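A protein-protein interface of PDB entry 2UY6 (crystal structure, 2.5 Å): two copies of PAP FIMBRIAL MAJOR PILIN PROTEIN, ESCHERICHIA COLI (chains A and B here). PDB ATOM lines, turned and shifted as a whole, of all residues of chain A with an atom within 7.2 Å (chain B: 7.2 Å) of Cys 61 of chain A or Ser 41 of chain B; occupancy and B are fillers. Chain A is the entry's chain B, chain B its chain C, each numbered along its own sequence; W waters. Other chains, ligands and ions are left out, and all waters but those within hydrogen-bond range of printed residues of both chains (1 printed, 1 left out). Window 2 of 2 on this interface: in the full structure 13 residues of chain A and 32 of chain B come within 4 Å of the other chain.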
ATOM      1  N   VAL A  17     -25.270  17.888 -22.628  1.00  0.00           N
ATOM      2  CA  VAL A  17     -24.521  19.068 -22.199  1.00  0.00           C
ATOM      3  C   VAL A  17     -23.843  18.841 -20.848  1.00  0.00           C
ATOM      4  O   VAL A  17     -24.468  18.392 -19.879  1.00  0.00           O
ATOM      5  CB  VAL A  17     -25.422  20.317 -22.082  1.00  0.00           C
ATOM      6  CG1 VAL A  17     -24.586  21.511 -21.641  1.00  0.00           C
ATOM      7  CG2 VAL A  17     -26.078  20.619 -23.416  1.00  0.00           C
ATOM      8  N   VAL A  18     -22.557  19.158 -20.792  1.00  0.00           N
ATOM      9  CA  VAL A  18     -21.794  18.986 -19.570  1.00  0.00           C
ATOM     10  C   VAL A  18     -20.993  20.238 -19.251  1.00  0.00           C
ATOM     11  O   VAL A  18     -20.780  21.093 -20.110  1.00  0.00           O
ATOM     12  CB  VAL A  18     -20.796  17.820 -19.695  1.00  0.00           C
ATOM     13  CG1 VAL A  18     -21.537  16.524 -19.965  1.00  0.00           C
ATOM     14  CG2 VAL A  18     -19.780  18.131 -20.800  1.00  0.00           C
ATOM     15  N   ASP A  19     -20.556  20.323 -18.001  1.00  0.00           N
ATOM     16  CA  ASP A  19     -19.745  21.428 -17.533  1.00  0.00           C
ATOM     17  C   ASP A  19     -18.310  21.027 -17.888  1.00  0.00           C
ATOM     18  O   ASP A  19     -17.847  19.956 -17.498  1.00  0.00           O
ATOM     19  CB  ASP A  19     -19.899  21.562 -16.025  1.00  0.00           C
ATOM     20  CG  ASP A  19     -19.321  22.848 -15.499  1.00  0.00           C
ATOM     21  OD1 ASP A  19     -18.959  22.884 -14.305  1.00  0.00           O
ATOM     22  OD2 ASP A  19     -19.241  23.821 -16.273  1.00  0.00           O
ATOM     23  N   ALA A  20     -17.620  21.873 -18.642  1.00  0.00           N
ATOM     24  CA  ALA A  20     -16.256  21.571 -19.067  1.00  0.00           C
ATOM     25  C   ALA A  20     -15.222  22.030 -18.044  1.00  0.00           C
ATOM     26  O   ALA A  20     -15.436  23.015 -17.345  1.00  0.00           O
ATOM     27  CB  ALA A  20     -15.977  22.226 -20.435  1.00  0.00           C
ATOM     28  N   PRO A  21     -14.090  21.310 -17.938  1.00  0.00           N
ATOM     29  CA  PRO A  21     -13.042  21.686 -16.984  1.00  0.00           C
ATOM     30  C   PRO A  21     -12.323  22.891 -17.571  1.00  0.00           C
ATOM     31  O   PRO A  21     -12.398  23.131 -18.779  1.00  0.00           O
ATOM     32  CB  PRO A  21     -12.129  20.462 -16.948  1.00  0.00           C
ATOM     33  CG  PRO A  21     -12.915  19.368 -17.631  1.00  0.00           C
ATOM     34  CD  PRO A  21     -13.706  20.095 -18.669  1.00  0.00           C
ATOM     35  N   CYS A  22     -11.622  23.649 -16.738  1.00  0.00           N
ATOM     36  CA  CYS A  22     -10.920  24.818 -17.240  1.00  0.00           C
ATOM     37  C   CYS A  22      -9.648  24.516 -18.037  1.00  0.00           C
ATOM     38  O   CYS A  22      -8.968  23.513 -17.815  1.00  0.00           O
ATOM     39  CB  CYS A  22     -10.589  25.772 -16.091  1.00  0.00           C
ATOM     40  SG  CYS A  22     -12.042  26.622 -15.400  1.00  0.00           S
ATOM     41  N   SER A  23      -9.356  25.401 -18.982  1.00  0.00           N
ATOM     42  CA  SER A  23      -8.170  25.311 -19.815  1.00  0.00           C
ATOM     43  C   SER A  23      -7.381  26.583 -19.485  1.00  0.00           C
ATOM     44  O   SER A  23      -7.985  27.623 -19.213  1.00  0.00           O
ATOM     45  CB  SER A  23      -8.574  25.300 -21.290  1.00  0.00           C
ATOM     46  OG  SER A  23      -7.446  25.161 -22.133  1.00  0.00           O
ATOM     47  N   LEU A  58      -8.039  31.564 -17.390  1.00  0.00           N
ATOM     48  CA  LEU A  58      -8.929  30.404 -17.350  1.00  0.00           C
ATOM     49  C   LEU A  58      -9.911  30.522 -18.508  1.00  0.00           C
ATOM     50  O   LEU A  58     -10.713  31.451 -18.545  1.00  0.00           O
ATOM     51  CB  LEU A  58      -9.701  30.367 -16.027  1.00  0.00           C
ATOM     52  CG  LEU A  58      -8.799  30.297 -14.792  1.00  0.00           C
ATOM     53  CD1 LEU A  58      -9.613  30.355 -13.502  1.00  0.00           C
ATOM     54  CD2 LEU A  58      -8.000  29.021 -14.857  1.00  0.00           C
ATOM     55  N   VAL A  59      -9.842  29.593 -19.458  1.00  0.00           N
ATOM     56  CA  VAL A  59     -10.739  29.626 -20.613  1.00  0.00           C
ATOM     57  C   VAL A  59     -11.541  28.339 -20.815  1.00  0.00           C
ATOM     58  O   VAL A  59     -11.317  27.330 -20.143  1.00  0.00           O
ATOM     59  CB  VAL A  59      -9.956  29.921 -21.909  1.00  0.00           C
ATOM     60  CG1 VAL A  59      -9.258  31.257 -21.790  1.00  0.00           C
ATOM     61  CG2 VAL A  59      -8.937  28.815 -22.180  1.00  0.00           C
ATOM     62  N   ASN A  60     -12.484  28.396 -21.749  1.00  0.00           N
ATOM     63  CA  ASN A  60     -13.343  27.264 -22.086  1.00  0.00           C
ATOM     64  C   ASN A  60     -14.060  26.638 -20.898  1.00  0.00           C
ATOM     65  O   ASN A  60     -14.366  25.450 -20.915  1.00  0.00           O
ATOM     66  CB  ASN A  60     -12.545  26.184 -22.821  1.00  0.00           C
ATOM     67  CG  ASN A  60     -11.839  26.721 -24.054  1.00  0.00           C
ATOM     68  OD1 ASN A  60     -12.323  27.647 -24.705  1.00  0.00           O
ATOM     69  ND2 ASN A  60     -10.695  26.133 -24.386  1.00  0.00           N
ATOM     70  N   CYS A  61     -14.333  27.429 -19.871  1.00  0.00           N
ATOM     71  CA  CYS A  61     -15.044  26.910 -18.712  1.00  0.00           C
ATOM     72  C   CYS A  61     -15.875  28.013 -18.078  1.00  0.00           C
ATOM     73  O   CYS A  61     -15.818  29.168 -18.506  1.00  0.00           O
ATOM     74  CB  CYS A  61     -14.062  26.350 -17.680  1.00  0.00           C
ATOM     75  SG  CYS A  61     -12.888  27.569 -17.003  1.00  0.00           S
ATOM     76  N   ASP A  62     -16.666  27.645 -17.072  1.00  0.00           N
ATOM     77  CA  ASP A  62     -17.488  28.607 -16.356  1.00  0.00           C
ATOM     78  C   ASP A  62     -16.623  29.008 -15.183  1.00  0.00           C
ATOM     79  O   ASP A  62     -16.379  28.205 -14.286  1.00  0.00           O
ATOM     80  CB  ASP A  62     -18.783  27.958 -15.871  1.00  0.00           C
ATOM     81  N   ILE A  63     -16.146  30.246 -15.207  1.00  0.00           N
ATOM     82  CA  ILE A  63     -15.274  30.759 -14.159  1.00  0.00           C
ATOM     83  C   ILE A  63     -15.996  31.031 -12.844  1.00  0.00           C
ATOM     84  O   ILE A  63     -15.374  31.437 -11.860  1.00  0.00           O
ATOM     85  CB  ILE A  63     -14.563  32.053 -14.626  1.00  0.00           C
ATOM     86  N   THR A  64     -17.305  30.797 -12.832  1.00  0.00           N
ATOM     87  CA  THR A  64     -18.124  31.022 -11.640  1.00  0.00           C
ATOM     88  C   THR A  64     -17.840  29.989 -10.565  1.00  0.00           C
ATOM     89  O   THR A  64     -18.761  29.471  -9.937  1.00  0.00           O
ATOM     90  CB  THR A  64     -19.629  30.953 -11.973  1.00  0.00           C
ATOM     91  OG1 THR A  64     -19.931  29.664 -12.526  1.00  0.00           O
ATOM     92  CG2 THR A  64     -20.011  32.041 -12.975  1.00  0.00           C
ATOM     93  N   PHE A  66     -14.196  30.117  -9.418  1.00  0.00           N
ATOM     94  CA  PHE A  66     -12.927  30.667  -8.956  1.00  0.00           C
ATOM     95  C   PHE A  66     -13.158  32.121  -8.549  1.00  0.00           C
ATOM     96  O   PHE A  66     -12.246  32.803  -8.088  1.00  0.00           O
ATOM     97  CB  PHE A  66     -11.869  30.636 -10.071  1.00  0.00           C
ATOM     98  CG  PHE A  66     -11.604  29.266 -10.640  1.00  0.00           C
ATOM     99  CD1 PHE A  66     -12.443  28.723 -11.603  1.00  0.00           C
ATOM    100  CD2 PHE A  66     -10.495  28.533 -10.229  1.00  0.00           C
ATOM    101  CE1 PHE A  66     -12.180  27.475 -12.152  1.00  0.00           C
ATOM    102  CE2 PHE A  66     -10.226  27.289 -10.770  1.00  0.00           C
ATOM    103  CZ  PHE A  66     -11.069  26.757 -11.733  1.00  0.00           C
ATOM    104  N   ASN A 129     -11.148  36.753 -15.853  1.00  0.00           N
ATOM    105  CA  ASN A 129     -10.985  35.304 -15.920  1.00  0.00           C
ATOM    106  C   ASN A 129      -9.500  34.951 -15.819  1.00  0.00           C
ATOM    107  O   ASN A 129      -9.067  33.875 -16.241  1.00  0.00           O
ATOM    108  CB  ASN A 129     -11.560  34.770 -17.232  1.00  0.00           C
ATOM    109  CG  ASN A 129     -10.824  35.298 -18.441  1.00  0.00           C
ATOM    110  OD1 ASN A 129     -10.694  36.508 -18.618  1.00  0.00           O
ATOM    111  ND2 ASN A 129     -10.331  34.395 -19.278  1.00  0.00           N
ATOM    112  N   LEU A 160      -5.591  21.474 -10.971  1.00  0.00           N
ATOM    113  CA  LEU A 160      -7.006  21.747 -10.734  1.00  0.00           C
ATOM    114  C   LEU A 160      -7.705  20.404 -10.535  1.00  0.00           C
ATOM    115  O   LEU A 160      -7.782  19.591 -11.465  1.00  0.00           O
ATOM    116  CB  LEU A 160      -7.621  22.471 -11.934  1.00  0.00           C
ATOM    117  CG  LEU A 160      -7.011  23.838 -12.246  1.00  0.00           C
ATOM    118  CD1 LEU A 160      -7.730  24.486 -13.423  1.00  0.00           C
ATOM    119  CD2 LEU A 160      -7.108  24.713 -11.002  1.00  0.00           C
ATOM    120  N   TYR A 162     -11.186  18.712  -9.689  1.00  0.00           N
ATOM    121  CA  TYR A 162     -12.620  18.906  -9.578  1.00  0.00           C
ATOM    122  C   TYR A 162     -13.334  17.918  -8.684  1.00  0.00           C
ATOM    123  O   TYR A 162     -12.978  16.745  -8.609  1.00  0.00           O
ATOM    124  CB  TYR A 162     -13.266  18.862 -10.962  1.00  0.00           C
ATOM    125  CG  TYR A 162     -12.707  19.894 -11.891  1.00  0.00           C
ATOM    126  CD1 TYR A 162     -11.424  19.751 -12.424  1.00  0.00           C
ATOM    127  CD2 TYR A 162     -13.423  21.048 -12.190  1.00  0.00           C
ATOM    128  CE1 TYR A 162     -10.864  20.735 -13.228  1.00  0.00           C
ATOM    129  CE2 TYR A 162     -12.870  22.049 -12.996  1.00  0.00           C
ATOM    130  CZ  TYR A 162     -11.592  21.884 -13.509  1.00  0.00           C
ATOM    131  OH  TYR A 162     -11.027  22.869 -14.287  1.00  0.00           O
ATOM    132  N   LEU B  38     -21.784  18.186 -25.523  1.00  0.00           N
ATOM    133  CA  LEU B  38     -21.387  19.573 -25.713  1.00  0.00           C
ATOM    134  C   LEU B  38     -21.060  20.294 -24.413  1.00  0.00           C
ATOM    135  O   LEU B  38     -21.548  19.930 -23.335  1.00  0.00           O
ATOM    136  CB  LEU B  38     -22.493  20.340 -26.438  1.00  0.00           C
ATOM    137  CG  LEU B  38     -22.953  19.696 -27.739  1.00  0.00           C
ATOM    138  CD1 LEU B  38     -24.253  20.334 -28.196  1.00  0.00           C
ATOM    139  CD2 LEU B  38     -21.868  19.839 -28.779  1.00  0.00           C
ATOM    140  N   SER B  39     -20.238  21.334 -24.547  1.00  0.00           N
ATOM    141  CA  SER B  39     -19.802  22.168 -23.431  1.00  0.00           C
ATOM    142  C   SER B  39     -20.824  23.252 -23.102  1.00  0.00           C
ATOM    143  O   SER B  39     -21.217  24.026 -23.974  1.00  0.00           O
ATOM    144  CB  SER B  39     -18.467  22.829 -23.775  1.00  0.00           C
ATOM    145  OG  SER B  39     -18.128  23.830 -22.835  1.00  0.00           O
ATOM    146  N   LYS B  40     -21.256  23.303 -21.845  1.00  0.00           N
ATOM    147  CA  LYS B  40     -22.203  24.321 -21.415  1.00  0.00           C
ATOM    148  C   LYS B  40     -21.638  25.697 -21.775  1.00  0.00           C
ATOM    149  O   LYS B  40     -22.338  26.529 -22.354  1.00  0.00           O
ATOM    150  CB  LYS B  40     -22.433  24.233 -19.901  1.00  0.00           C
ATOM    151  CG  LYS B  40     -23.311  25.347 -19.353  1.00  0.00           C
ATOM    152  CD  LYS B  40     -23.641  25.182 -17.866  1.00  0.00           C
ATOM    153  CE  LYS B  40     -22.456  25.475 -16.942  1.00  0.00           C
ATOM    154  NZ  LYS B  40     -22.864  25.370 -15.497  1.00  0.00           N
ATOM    155  N   SER B  41     -20.365  25.914 -21.430  1.00  0.00           N
ATOM    156  CA  SER B  41     -19.662  27.169 -21.702  1.00  0.00           C
ATOM    157  C   SER B  41     -19.731  27.579 -23.166  1.00  0.00           C
ATOM    158  O   SER B  41     -20.107  28.705 -23.487  1.00  0.00           O
ATOM    159  CB  SER B  41     -18.183  27.051 -21.316  1.00  0.00           C
ATOM    160  OG  SER B  41     -18.020  27.091 -19.920  1.00  0.00           O
ATOM    161  N   PHE B  42     -19.328  26.665 -24.040  1.00  0.00           N
ATOM    162  CA  PHE B  42     -19.329  26.904 -25.472  1.00  0.00           C
ATOM    163  C   PHE B  42     -20.695  27.413 -25.935  1.00  0.00           C
ATOM    164  O   PHE B  42     -20.788  28.439 -26.616  1.00  0.00           O
ATOM    165  CB  PHE B  42     -18.990  25.605 -26.187  1.00  0.00           C
ATOM    166  CG  PHE B  42     -19.018  25.700 -27.680  1.00  0.00           C
ATOM    167  CD1 PHE B  42     -17.980  26.313 -28.371  1.00  0.00           C
ATOM    168  CD2 PHE B  42     -20.059  25.126 -28.402  1.00  0.00           C
ATOM    169  CE1 PHE B  42     -17.971  26.348 -29.767  1.00  0.00           C
ATOM    170  CE2 PHE B  42     -20.063  25.156 -29.802  1.00  0.00           C
ATOM    171  CZ  PHE B  42     -19.012  25.769 -30.484  1.00  0.00           C
ATOM    172  N   LEU B  43     -21.747  26.689 -25.555  1.00  0.00           N
ATOM    173  CA  LEU B  43     -23.116  27.045 -25.922  1.00  0.00           C
ATOM    174  C   LEU B  43     -23.542  28.404 -25.370  1.00  0.00           C
ATOM    175  O   LEU B  43     -24.001  29.272 -26.116  1.00  0.00           O
ATOM    176  CB  LEU B  43     -24.092  25.960 -25.431  1.00  0.00           C
ATOM    177  CG  LEU B  43     -24.483  24.801 -26.365  1.00  0.00           C
ATOM    178  CD1 LEU B  43     -23.493  24.657 -27.494  1.00  0.00           C
ATOM    179  CD2 LEU B  43     -24.572  23.510 -25.561  1.00  0.00           C
ATOM    180  N   GLU B  44     -23.381  28.581 -24.064  1.00  0.00           N
ATOM    181  CA  GLU B  44     -23.761  29.816 -23.396  1.00  0.00           C
ATOM    182  C   GLU B  44     -23.053  31.047 -23.948  1.00  0.00           C
ATOM    183  O   GLU B  44     -23.578  32.153 -23.855  1.00  0.00           O
ATOM    184  CB  GLU B  44     -23.488  29.702 -21.896  1.00  0.00           C
ATOM    185  CG  GLU B  44     -24.041  30.849 -21.080  1.00  0.00           C
ATOM    186  CD  GLU B  44     -25.548  30.983 -21.204  1.00  0.00           C
ATOM    187  OE1 GLU B  44     -26.255  29.976 -20.995  1.00  0.00           O
ATOM    188  OE2 GLU B  44     -26.030  32.096 -21.505  1.00  0.00           O
ATOM    189  N   ALA B  45     -21.868  30.858 -24.516  1.00  0.00           N
ATOM    190  CA  ALA B  45     -21.110  31.970 -25.077  1.00  0.00           C
ATOM    191  C   ALA B  45     -21.391  32.131 -26.567  1.00  0.00           C
ATOM    192  O   ALA B  45     -20.622  32.783 -27.285  1.00  0.00           O
ATOM    193  CB  ALA B  45     -19.625  31.763 -24.848  1.00  0.00           C
ATOM    194  N   GLY B  46     -22.485  31.522 -27.029  1.00  0.00           N
ATOM    195  CA  GLY B  46     -22.870  31.630 -28.428  1.00  0.00           C
ATOM    196  C   GLY B  46     -22.308  30.575 -29.364  1.00  0.00           C
ATOM    197  O   GLY B  46     -22.485  30.658 -30.585  1.00  0.00           O
ATOM    198  N   GLY B  47     -21.625  29.582 -28.804  1.00  0.00           N
ATOM    199  CA  GLY B  47     -21.066  28.528 -29.630  1.00  0.00           C
ATOM    200  C   GLY B  47     -22.131  27.686 -30.316  1.00  0.00           C
ATOM    201  O   GLY B  47     -23.217  27.470 -29.775  1.00  0.00           O
ATOM    202  N   VAL B 147     -28.405  28.048 -20.797  1.00  0.00           N
ATOM    203  CA  VAL B 147     -27.980  26.683 -21.068  1.00  0.00           C
ATOM    204  C   VAL B 147     -27.666  25.918 -19.781  1.00  0.00           C
ATOM    205  O   VAL B 147     -26.872  26.367 -18.960  1.00  0.00           O
ATOM    206  CB  VAL B 147     -26.724  26.670 -21.962  1.00  0.00           C
ATOM    207  CG1 VAL B 147     -26.337  25.242 -22.284  1.00  0.00           C
ATOM    208  CG2 VAL B 147     -26.979  27.460 -23.231  1.00  0.00           C
HETATM  209  O   HOH W   1     -15.440  24.387 -23.476  1.00  0.00           O
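Among the printed residues, merely in contact across the chains: Val 17 of chain A with Leu 38 of chain B (3.3 Å), Val 17 of chain A with Lys 40 of chain B (3.7 Å), Val 17 of chain A with Leu 43 of chain B (3.9 Å), Val 18 of chain A with Ser 39 of chain B (3.6 Å), Asp 19 of chain A with Lys 40 of chain B (3.7 Å) and Ala 20 of chain A with Ser 39 of chain B (3.6 Å).
Water W1 bridges the side-chain hydroxyl of Ser 39 of chain B and the backbone carbonyl oxygen of Asn 60 of chain A.
OG of Ser 39 of chain B is in hydrogen-bond range of N of Phe 42 of chain B, 3.3 Å away. The side-chain hydroxyl of Ser 39 of chain B sits close to the backbone NH of Ser 41 of chain B (3.4 Å). SG of Cys 22 of chain A forms a disulfide with SG of Cys 61 of chain A (2.0 Å).
Printed residues of chain A that touch a printed residue of chain B: Val 17, Val 18, Asp 19, Ala 20, Cys 61 and Asp 62. Hydrophobic or aromatic side chains of chain A that line the printed part of chain B: Val 17, Val 18 and Ala 20. Hydrophobic or aromatic side chains of chain B within 4 Å of the printed part of chain A: Leu 43. Along chain B the printed residues that touch a printed residue of chain A span positions 38 to 43.
No position is printed for both chains.
Of the printed residues of chain B, Val 18 of chain A touches Leu 38, Ser 39 and Lys 40. Of the printed residues of chain B, Ala 20 of chain A touches Ser 39. Of chain B, only Ser 41 comes within 4 Å of Cys 61 of chain A. Ser 41 of chain B touches just these residues of chain A: Cys 61 and Asp 62. The nearest residue of chain A that does not touch Ser 41 of chain B is Asn 60 of chain A (4.1 Å). The nearest printed residue of chain A that does not touch Ser 39 of chain B is Val 17 of chain A (4.4 Å).
The side-chain hydroxyl (OG) of Ser 41 of chain B lies within hydrogen-bond range of the backbone NH (N) of Asp 62 of chain A (3.2 Å). The side-chain hydroxyl (OG) of Ser 41 of chain B sits close to the backbone carbonyl oxygen (O) of Cys 61 of chain A. N of Val 18 of chain A sits at hydrogen-bond distance from O of Leu 38 of chain B, 2.8 Å away. N of Lys 40 of chain B lies within hydrogen-bond range of O of Val 18 of chain A (2.8 Å).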
